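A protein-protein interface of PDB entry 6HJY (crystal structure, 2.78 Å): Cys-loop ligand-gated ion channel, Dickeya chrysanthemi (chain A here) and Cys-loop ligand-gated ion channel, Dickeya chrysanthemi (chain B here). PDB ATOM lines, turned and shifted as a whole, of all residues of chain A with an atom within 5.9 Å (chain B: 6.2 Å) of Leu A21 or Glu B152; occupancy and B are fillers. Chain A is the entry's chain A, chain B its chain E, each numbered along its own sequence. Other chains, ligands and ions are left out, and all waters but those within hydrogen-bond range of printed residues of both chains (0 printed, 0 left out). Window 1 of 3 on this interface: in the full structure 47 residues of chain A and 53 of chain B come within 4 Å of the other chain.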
ATOM      1  N   ASN A  19       2.813  37.914 -24.420  1.00  0.00           N
ATOM      2  CA  ASN A  19       2.497  36.504 -24.227  1.00  0.00           C
ATOM      3  C   ASN A  19       2.314  36.345 -22.722  1.00  0.00           C
ATOM      4  O   ASN A  19       3.295  36.312 -21.971  1.00  0.00           O
ATOM      5  CB  ASN A  19       3.612  35.595 -24.759  1.00  0.00           C
ATOM      6  CG  ASN A  19       3.317  34.111 -24.668  1.00  0.00           C
ATOM      7  OD1 ASN A  19       2.758  33.608 -23.687  1.00  0.00           O
ATOM      8  ND2 ASN A  19       3.748  33.360 -25.671  1.00  0.00           N
ATOM      9  N   THR A  20       1.048  36.309 -22.290  1.00  0.00           N
ATOM     10  CA  THR A  20       0.637  36.203 -20.887  1.00  0.00           C
ATOM     11  C   THR A  20       1.227  34.998 -20.147  1.00  0.00           C
ATOM     12  O   THR A  20       1.751  35.158 -19.041  1.00  0.00           O
ATOM     13  CB  THR A  20      -0.892  36.212 -20.759  1.00  0.00           C
ATOM     14  OG1 THR A  20      -1.426  35.195 -21.604  1.00  0.00           O
ATOM     15  CG2 THR A  20      -1.506  37.564 -21.090  1.00  0.00           C
ATOM     16  N   LEU A  21       1.153  33.803 -20.753  1.00  0.00           N
ATOM     17  CA  LEU A  21       1.649  32.585 -20.115  1.00  0.00           C
ATOM     18  C   LEU A  21       3.170  32.523 -20.014  1.00  0.00           C
ATOM     19  O   LEU A  21       3.689  32.014 -19.018  1.00  0.00           O
ATOM     20  CB  LEU A  21       1.077  31.327 -20.784  1.00  0.00           C
ATOM     21  CG  LEU A  21       1.053  30.041 -19.930  1.00  0.00           C
ATOM     22  CD1 LEU A  21       0.476  30.287 -18.520  1.00  0.00           C
ATOM     23  CD2 LEU A  21       0.287  28.931 -20.642  1.00  0.00           C
ATOM     24  N   GLU A  22       3.886  33.062 -21.016  1.00  0.00           N
ATOM     25  CA  GLU A  22       5.351  33.085 -21.021  1.00  0.00           C
ATOM     26  C   GLU A  22       5.915  34.282 -20.276  1.00  0.00           C
ATOM     27  O   GLU A  22       7.107  34.287 -19.963  1.00  0.00           O
ATOM     28  CB  GLU A  22       5.900  33.066 -22.452  1.00  0.00           C
ATOM     29  CG  GLU A  22       5.806  31.706 -23.123  1.00  0.00           C
ATOM     30  CD  GLU A  22       6.624  31.541 -24.391  1.00  0.00           C
ATOM     31  OE1 GLU A  22       7.140  32.555 -24.920  1.00  0.00           O
ATOM     32  OE2 GLU A  22       6.748  30.388 -24.863  1.00  0.00           O
ATOM     33  N   GLN A  23       5.058  35.297 -20.001  1.00  0.00           N
ATOM     34  CA  GLN A  23       5.400  36.569 -19.348  1.00  0.00           C
ATOM     35  C   GLN A  23       6.479  37.315 -20.149  1.00  0.00           C
ATOM     36  O   GLN A  23       7.467  37.797 -19.593  1.00  0.00           O
ATOM     37  CB  GLN A  23       5.761  36.386 -17.863  1.00  0.00           C
ATOM     38  CG  GLN A  23       4.552  36.285 -16.945  1.00  0.00           C
ATOM     39  CD  GLN A  23       4.977  35.971 -15.539  1.00  0.00           C
ATOM     40  OE1 GLN A  23       5.305  36.856 -14.748  1.00  0.00           O
ATOM     41  NE2 GLN A  23       5.022  34.695 -15.205  1.00  0.00           N
ATOM     42  N   PHE A 108      -1.433  39.377 -14.339  1.00  0.00           N
ATOM     43  CA  PHE A 108      -2.659  39.615 -15.094  1.00  0.00           C
ATOM     44  C   PHE A 108      -3.933  39.285 -14.307  1.00  0.00           C
ATOM     45  O   PHE A 108      -4.989  39.140 -14.919  1.00  0.00           O
ATOM     46  CB  PHE A 108      -2.634  38.824 -16.413  1.00  0.00           C
ATOM     47  CG  PHE A 108      -1.430  39.061 -17.289  1.00  0.00           C
ATOM     48  CD1 PHE A 108      -1.386  40.144 -18.156  1.00  0.00           C
ATOM     49  CD2 PHE A 108      -0.357  38.181 -17.274  1.00  0.00           C
ATOM     50  CE1 PHE A 108      -0.275  40.354 -18.972  1.00  0.00           C
ATOM     51  CE2 PHE A 108       0.747  38.390 -18.093  1.00  0.00           C
ATOM     52  CZ  PHE A 108       0.778  39.472 -18.940  1.00  0.00           C
ATOM     53  N   ARG A 247      -4.254  32.673 -22.070  1.00  0.00           N
ATOM     54  CA  ARG A 247      -3.922  31.508 -21.241  1.00  0.00           C
ATOM     55  C   ARG A 247      -3.183  31.955 -19.985  1.00  0.00           C
ATOM     56  O   ARG A 247      -2.160  32.641 -20.080  1.00  0.00           O
ATOM     57  CB  ARG A 247      -3.099  30.459 -22.026  1.00  0.00           C
ATOM     58  CG  ARG A 247      -3.775  29.917 -23.288  1.00  0.00           C
ATOM     59  CD  ARG A 247      -4.966  29.015 -22.979  1.00  0.00           C
ATOM     60  NE  ARG A 247      -5.542  28.461 -24.205  1.00  0.00           N
ATOM     61  CZ  ARG A 247      -6.527  29.020 -24.906  1.00  0.00           C
ATOM     62  NH1 ARG A 247      -7.075  30.162 -24.502  1.00  0.00           N
ATOM     63  NH2 ARG A 247      -6.979  28.436 -26.008  1.00  0.00           N
ATOM     64  N   LEU A 248      -3.734  31.612 -18.805  1.00  0.00           N
ATOM     65  CA  LEU A 248      -3.163  32.006 -17.517  1.00  0.00           C
ATOM     66  C   LEU A 248      -3.201  30.892 -16.456  1.00  0.00           C
ATOM     67  O   LEU A 248      -4.119  30.070 -16.473  1.00  0.00           O
ATOM     68  CB  LEU A 248      -3.859  33.281 -16.997  1.00  0.00           C
ATOM     69  CG  LEU A 248      -3.490  34.599 -17.687  1.00  0.00           C
ATOM     70  CD1 LEU A 248      -4.500  35.659 -17.385  1.00  0.00           C
ATOM     71  CD2 LEU A 248      -2.098  35.068 -17.284  1.00  0.00           C
ATOM     72  N   PRO A 249      -2.235  30.850 -15.501  1.00  0.00           N
ATOM     73  CA  PRO A 249      -2.274  29.797 -14.470  1.00  0.00           C
ATOM     74  C   PRO A 249      -3.161  30.143 -13.261  1.00  0.00           C
ATOM     75  O   PRO A 249      -3.190  29.401 -12.277  1.00  0.00           O
ATOM     76  CB  PRO A 249      -0.807  29.667 -14.071  1.00  0.00           C
ATOM     77  CG  PRO A 249      -0.244  31.041 -14.259  1.00  0.00           C
ATOM     78  CD  PRO A 249      -1.068  31.744 -15.309  1.00  0.00           C
ATOM     79  N   TYR B  17      10.106  27.563 -18.824  1.00  0.00           N
ATOM     80  CA  TYR B  17       8.792  27.917 -19.343  1.00  0.00           C
ATOM     81  C   TYR B  17       8.497  27.153 -20.640  1.00  0.00           C
ATOM     82  O   TYR B  17       9.269  26.278 -21.024  1.00  0.00           O
ATOM     83  CB  TYR B  17       8.754  29.448 -19.578  1.00  0.00           C
ATOM     84  CG  TYR B  17       9.594  29.908 -20.753  1.00  0.00           C
ATOM     85  CD1 TYR B  17      10.987  29.982 -20.653  1.00  0.00           C
ATOM     86  CD2 TYR B  17       9.009  30.279 -21.954  1.00  0.00           C
ATOM     87  CE1 TYR B  17      11.765  30.397 -21.737  1.00  0.00           C
ATOM     88  CE2 TYR B  17       9.776  30.685 -23.044  1.00  0.00           C
ATOM     89  CZ  TYR B  17      11.153  30.750 -22.929  1.00  0.00           C
ATOM     90  OH  TYR B  17      11.885  31.138 -24.017  1.00  0.00           O
ATOM     91  N   GLY B  18       7.384  27.496 -21.284  1.00  0.00           N
ATOM     92  CA  GLY B  18       6.953  26.935 -22.562  1.00  0.00           C
ATOM     93  C   GLY B  18       6.880  25.426 -22.630  1.00  0.00           C
ATOM     94  O   GLY B  18       7.344  24.840 -23.615  1.00  0.00           O
ATOM     95  N   VAL B  19       6.305  24.789 -21.579  1.00  0.00           N
ATOM     96  CA  VAL B  19       6.136  23.331 -21.523  1.00  0.00           C
ATOM     97  C   VAL B  19       5.198  22.918 -22.652  1.00  0.00           C
ATOM     98  O   VAL B  19       4.177  23.573 -22.877  1.00  0.00           O
ATOM     99  CB  VAL B  19       5.662  22.803 -20.133  1.00  0.00           C
ATOM    100  CG1 VAL B  19       5.361  21.303 -20.167  1.00  0.00           C
ATOM    101  CG2 VAL B  19       6.692  23.103 -19.047  1.00  0.00           C
ATOM    102  N   GLU B 148       5.223  33.193  -6.173  1.00  0.00           N
ATOM    103  CA  GLU B 148       4.927  32.072  -7.066  1.00  0.00           C
ATOM    104  C   GLU B 148       3.454  32.014  -7.501  1.00  0.00           C
ATOM    105  O   GLU B 148       3.127  31.257  -8.417  1.00  0.00           O
ATOM    106  CB  GLU B 148       5.388  30.738  -6.448  1.00  0.00           C
ATOM    107  CG  GLU B 148       4.768  30.414  -5.094  1.00  0.00           C
ATOM    108  CD  GLU B 148       4.983  28.999  -4.580  1.00  0.00           C
ATOM    109  OE1 GLU B 148       6.087  28.442  -4.774  1.00  0.00           O
ATOM    110  OE2 GLU B 148       4.055  28.459  -3.937  1.00  0.00           O
ATOM    111  N   GLU B 149       2.575  32.822  -6.847  1.00  0.00           N
ATOM    112  CA  GLU B 149       1.133  32.931  -7.133  1.00  0.00           C
ATOM    113  C   GLU B 149       0.895  33.255  -8.613  1.00  0.00           C
ATOM    114  O   GLU B 149       0.020  32.657  -9.240  1.00  0.00           O
ATOM    115  CB  GLU B 149       0.487  34.043  -6.283  1.00  0.00           C
ATOM    116  CG  GLU B 149       0.085  33.651  -4.873  1.00  0.00           C
ATOM    117  CD  GLU B 149      -0.665  34.761  -4.154  1.00  0.00           C
ATOM    118  OE1 GLU B 149      -0.029  35.782  -3.804  1.00  0.00           O
ATOM    119  OE2 GLU B 149      -1.897  34.631  -3.969  1.00  0.00           O
ATOM    120  N   ILE B 150       1.704  34.191  -9.162  1.00  0.00           N
ATOM    121  CA  ILE B 150       1.652  34.669 -10.547  1.00  0.00           C
ATOM    122  C   ILE B 150       2.369  33.713 -11.535  1.00  0.00           C
ATOM    123  O   ILE B 150       2.342  33.959 -12.745  1.00  0.00           O
ATOM    124  CB  ILE B 150       2.154  36.146 -10.676  1.00  0.00           C
ATOM    125  CG1 ILE B 150       3.695  36.266 -10.556  1.00  0.00           C
ATOM    126  CG2 ILE B 150       1.424  37.076  -9.688  1.00  0.00           C
ATOM    127  CD1 ILE B 150       4.334  37.314 -11.445  1.00  0.00           C
ATOM    128  N   ASP B 151       3.019  32.645 -11.014  1.00  0.00           N
ATOM    129  CA  ASP B 151       3.764  31.660 -11.805  1.00  0.00           C
ATOM    130  C   ASP B 151       3.002  30.353 -12.041  1.00  0.00           C
ATOM    131  O   ASP B 151       2.297  29.868 -11.153  1.00  0.00           O
ATOM    132  CB  ASP B 151       5.133  31.361 -11.161  1.00  0.00           C
ATOM    133  CG  ASP B 151       6.067  32.552 -11.050  1.00  0.00           C
ATOM    134  OD1 ASP B 151       6.141  33.343 -12.018  1.00  0.00           O
ATOM    135  OD2 ASP B 151       6.761  32.663 -10.021  1.00  0.00           O
ATOM    136  N   GLU B 152       3.203  29.765 -13.238  1.00  0.00           N
ATOM    137  CA  GLU B 152       2.594  28.511 -13.679  1.00  0.00           C
ATOM    138  C   GLU B 152       3.150  27.306 -12.915  1.00  0.00           C
ATOM    139  O   GLU B 152       2.398  26.382 -12.592  1.00  0.00           O
ATOM    140  CB  GLU B 152       2.776  28.335 -15.196  1.00  0.00           C
ATOM    141  CG  GLU B 152       1.891  27.255 -15.802  1.00  0.00           C
ATOM    142  CD  GLU B 152       2.039  27.007 -17.295  1.00  0.00           C
ATOM    143  OE1 GLU B 152       2.843  27.706 -17.955  1.00  0.00           O
ATOM    144  OE2 GLU B 152       1.338  26.107 -17.810  1.00  0.00           O
ATOM    145  N   TRP B 153       4.464  27.315 -12.647  1.00  0.00           N
ATOM    146  CA  TRP B 153       5.158  26.245 -11.937  1.00  0.00           C
ATOM    147  C   TRP B 153       5.700  26.717 -10.601  1.00  0.00           C
ATOM    148  O   TRP B 153       6.078  27.884 -10.457  1.00  0.00           O
ATOM    149  CB  TRP B 153       6.278  25.649 -12.806  1.00  0.00           C
ATOM    150  CG  TRP B 153       5.746  24.878 -13.978  1.00  0.00           C
ATOM    151  CD1 TRP B 153       5.566  25.339 -15.248  1.00  0.00           C
ATOM    152  CD2 TRP B 153       5.243  23.533 -13.961  1.00  0.00           C
ATOM    153  NE1 TRP B 153       5.008  24.356 -16.036  1.00  0.00           N
ATOM    154  CE2 TRP B 153       4.798  23.235 -15.270  1.00  0.00           C
ATOM    155  CE3 TRP B 153       5.145  22.542 -12.969  1.00  0.00           C
ATOM    156  CZ2 TRP B 153       4.257  21.985 -15.610  1.00  0.00           C
ATOM    157  CZ3 TRP B 153       4.605  21.308 -13.305  1.00  0.00           C
ATOM    158  CH2 TRP B 153       4.154  21.045 -14.605  1.00  0.00           C
ATOM    159  N   TRP B 154       5.714  25.809  -9.618  1.00  0.00           N
ATOM    160  CA  TRP B 154       6.203  26.086  -8.273  1.00  0.00           C
ATOM    161  C   TRP B 154       7.399  25.195  -7.955  1.00  0.00           C
ATOM    162  O   TRP B 154       7.227  24.001  -7.686  1.00  0.00           O
ATOM    163  CB  TRP B 154       5.087  25.888  -7.237  1.00  0.00           C
ATOM    164  CG  TRP B 154       3.900  26.805  -7.363  1.00  0.00           C
ATOM    165  CD1 TRP B 154       3.848  28.016  -7.991  1.00  0.00           C
ATOM    166  CD2 TRP B 154       2.612  26.606  -6.766  1.00  0.00           C
ATOM    167  NE1 TRP B 154       2.590  28.563  -7.864  1.00  0.00           N
ATOM    168  CE2 TRP B 154       1.816  27.725  -7.101  1.00  0.00           C
ATOM    169  CE3 TRP B 154       2.045  25.578  -5.991  1.00  0.00           C
ATOM    170  CZ2 TRP B 154       0.489  27.855  -6.665  1.00  0.00           C
ATOM    171  CZ3 TRP B 154       0.727  25.696  -5.580  1.00  0.00           C
ATOM    172  CH2 TRP B 154      -0.042  26.817  -5.925  1.00  0.00           C
ATOM    173  N   VAL B 191       6.054  21.726  -8.996  1.00  0.00           N
ATOM    174  CA  VAL B 191       4.651  21.323  -8.849  1.00  0.00           C
ATOM    175  C   VAL B 191       3.822  22.345  -9.633  1.00  0.00           C
ATOM    176  O   VAL B 191       4.117  23.542  -9.570  1.00  0.00           O
ATOM    177  CB  VAL B 191       4.229  21.279  -7.349  1.00  0.00           C
ATOM    178  CG1 VAL B 191       2.753  20.921  -7.187  1.00  0.00           C
ATOM    179  CG2 VAL B 191       5.098  20.307  -6.555  1.00  0.00           C
ATOM    180  N   ARG B 192       2.807  21.889 -10.384  1.00  0.00           N
ATOM    181  CA  ARG B 192       1.963  22.812 -11.142  1.00  0.00           C
ATOM    182  C   ARG B 192       1.052  23.620 -10.216  1.00  0.00           C
ATOM    183  O   ARG B 192       0.637  23.122  -9.166  1.00  0.00           O
ATOM    184  CB  ARG B 192       1.128  22.071 -12.200  1.00  0.00           C
ATOM    185  CG  ARG B 192       0.540  23.006 -13.265  1.00  0.00           C
ATOM    186  CD  ARG B 192      -0.447  22.317 -14.179  1.00  0.00           C
ATOM    187  NE  ARG B 192       0.184  21.214 -14.900  1.00  0.00           N
ATOM    188  CZ  ARG B 192       0.828  21.324 -16.060  1.00  0.00           C
ATOM    189  NH1 ARG B 192       0.924  22.507 -16.659  1.00  0.00           N
ATOM    190  NH2 ARG B 192       1.376  20.264 -16.627  1.00  0.00           N
ATOM    191  N   ASN B 193       0.781  24.881 -10.603  1.00  0.00           N
ATOM    192  CA  ASN B 193      -0.129  25.797  -9.921  1.00  0.00           C
ATOM    193  C   ASN B 193      -1.548  25.375 -10.378  1.00  0.00           C
ATOM    194  O   ASN B 193      -1.902  25.585 -11.546  1.00  0.00           O
ATOM    195  CB  ASN B 193       0.198  27.254 -10.325  1.00  0.00           C
ATOM    196  CG  ASN B 193      -0.650  28.345  -9.707  1.00  0.00           C
ATOM    197  OD1 ASN B 193      -1.688  28.112  -9.084  1.00  0.00           O
ATOM    198  ND2 ASN B 193      -0.191  29.578  -9.843  1.00  0.00           N
ATOM    199  N   PRO B 194      -2.350  24.714  -9.508  1.00  0.00           N
ATOM    200  CA  PRO B 194      -3.666  24.241  -9.954  1.00  0.00           C
ATOM    201  C   PRO B 194      -4.833  25.209  -9.738  1.00  0.00           C
ATOM    202  O   PRO B 194      -5.975  24.813  -9.972  1.00  0.00           O
ATOM    203  CB  PRO B 194      -3.840  22.953  -9.149  1.00  0.00           C
ATOM    204  CG  PRO B 194      -3.072  23.194  -7.874  1.00  0.00           C
ATOM    205  CD  PRO B 194      -2.103  24.331  -8.101  1.00  0.00           C
ATOM    206  N   TYR B 197      -7.434  25.694 -12.681  1.00  0.00           N
ATOM    207  CA  TYR B 197      -8.199  24.469 -12.935  1.00  0.00           C
ATOM    208  C   TYR B 197      -9.127  24.070 -11.791  1.00  0.00           C
ATOM    209  O   TYR B 197     -10.133  23.403 -12.036  1.00  0.00           O
ATOM    210  CB  TYR B 197      -7.262  23.318 -13.331  1.00  0.00           C
ATOM    211  CG  TYR B 197      -6.392  23.670 -14.522  1.00  0.00           C
ATOM    212  CD1 TYR B 197      -6.902  23.618 -15.819  1.00  0.00           C
ATOM    213  CD2 TYR B 197      -5.089  24.123 -14.352  1.00  0.00           C
ATOM    214  CE1 TYR B 197      -6.125  23.993 -16.915  1.00  0.00           C
ATOM    215  CE2 TYR B 197      -4.299  24.490 -15.441  1.00  0.00           C
ATOM    216  CZ  TYR B 197      -4.824  24.425 -16.722  1.00  0.00           C
ATOM    217  OH  TYR B 197      -4.050  24.783 -17.795  1.00  0.00           O
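Printed residues of chain B that touch a printed residue of chain A: Tyr B17, Ile B150, Asp B151, Glu B152 and Asn B193. Among the printed residues, 7 pairs touch across the chains. Among the printed residues, no Asp or Glu carboxylate lies within 4 Å of a Lys or Arg side-chain nitrogen of the other chain.
Of chain B, only Glu B152 (3.5 Å) comes within 4 Å of Leu A21. Glu B152 touches just these residues of chain A: Leu A21 and Pro A249. Printed residues of chain A within 4 Å of Asn B193: Pro A249. Of the printed residues of chain A, Asp B151 touches Gln A23 (3.6 Å) and Pro A249 (3.99 Å). Arg B192 touches none of the printed residues of chain A. The nearest residue of chain B that does not touch Leu A21 is Tyr B17 (5.7 Å). The nearest residue of chain A that does not touch Glu B152 is Gln A23 (5.6 Å). The nearest printed residue of chain A that does not touch Asn B193 is Leu A248 (7.0 Å).
The side-chain amide nitrogen (ND2) of Asn B193 is in hydrogen-bond range of the backbone carbonyl oxygen (O) of Glu B149 (3.1 Å). The backbone NH (N) of Glu A22 is in hydrogen-bond range of the side-chain amide oxygen (OD1) of Asn A19, at 3.0 Å. The guanidinium group (NH1) of Arg B192 lies within salt-bridge range of the side-chain carboxylate (OE2) of Glu B152, at 3.8 Å. N of Asn B193 is in hydrogen-bond range of O of Glu B152, at 3.0 Å. The backbone carbonyl oxygen (O) of Asp B151 sits at hydrogen-bond distance from the side-chain amide nitrogen (ND2) of Asn B193 (2.8 Å). N of Leu A21 sits at hydrogen-bond distance from OD1 of Asn A19 (3.3 Å).
Among the printed residues, merely in contact across the chains: Gln A23 with Ile B150 (3.5 Å), Glu A22 with Tyr B17 (3.5 Å), Leu A21 with Glu B152 (3.5 Å), Pro A249 with Glu B152 (3.6 Å), Gln A23 with Asp B151 (3.6 Å), Pro A249 with Asn B193 (3.8 Å) and Pro A249 with Asp B151 (3.99 Å).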
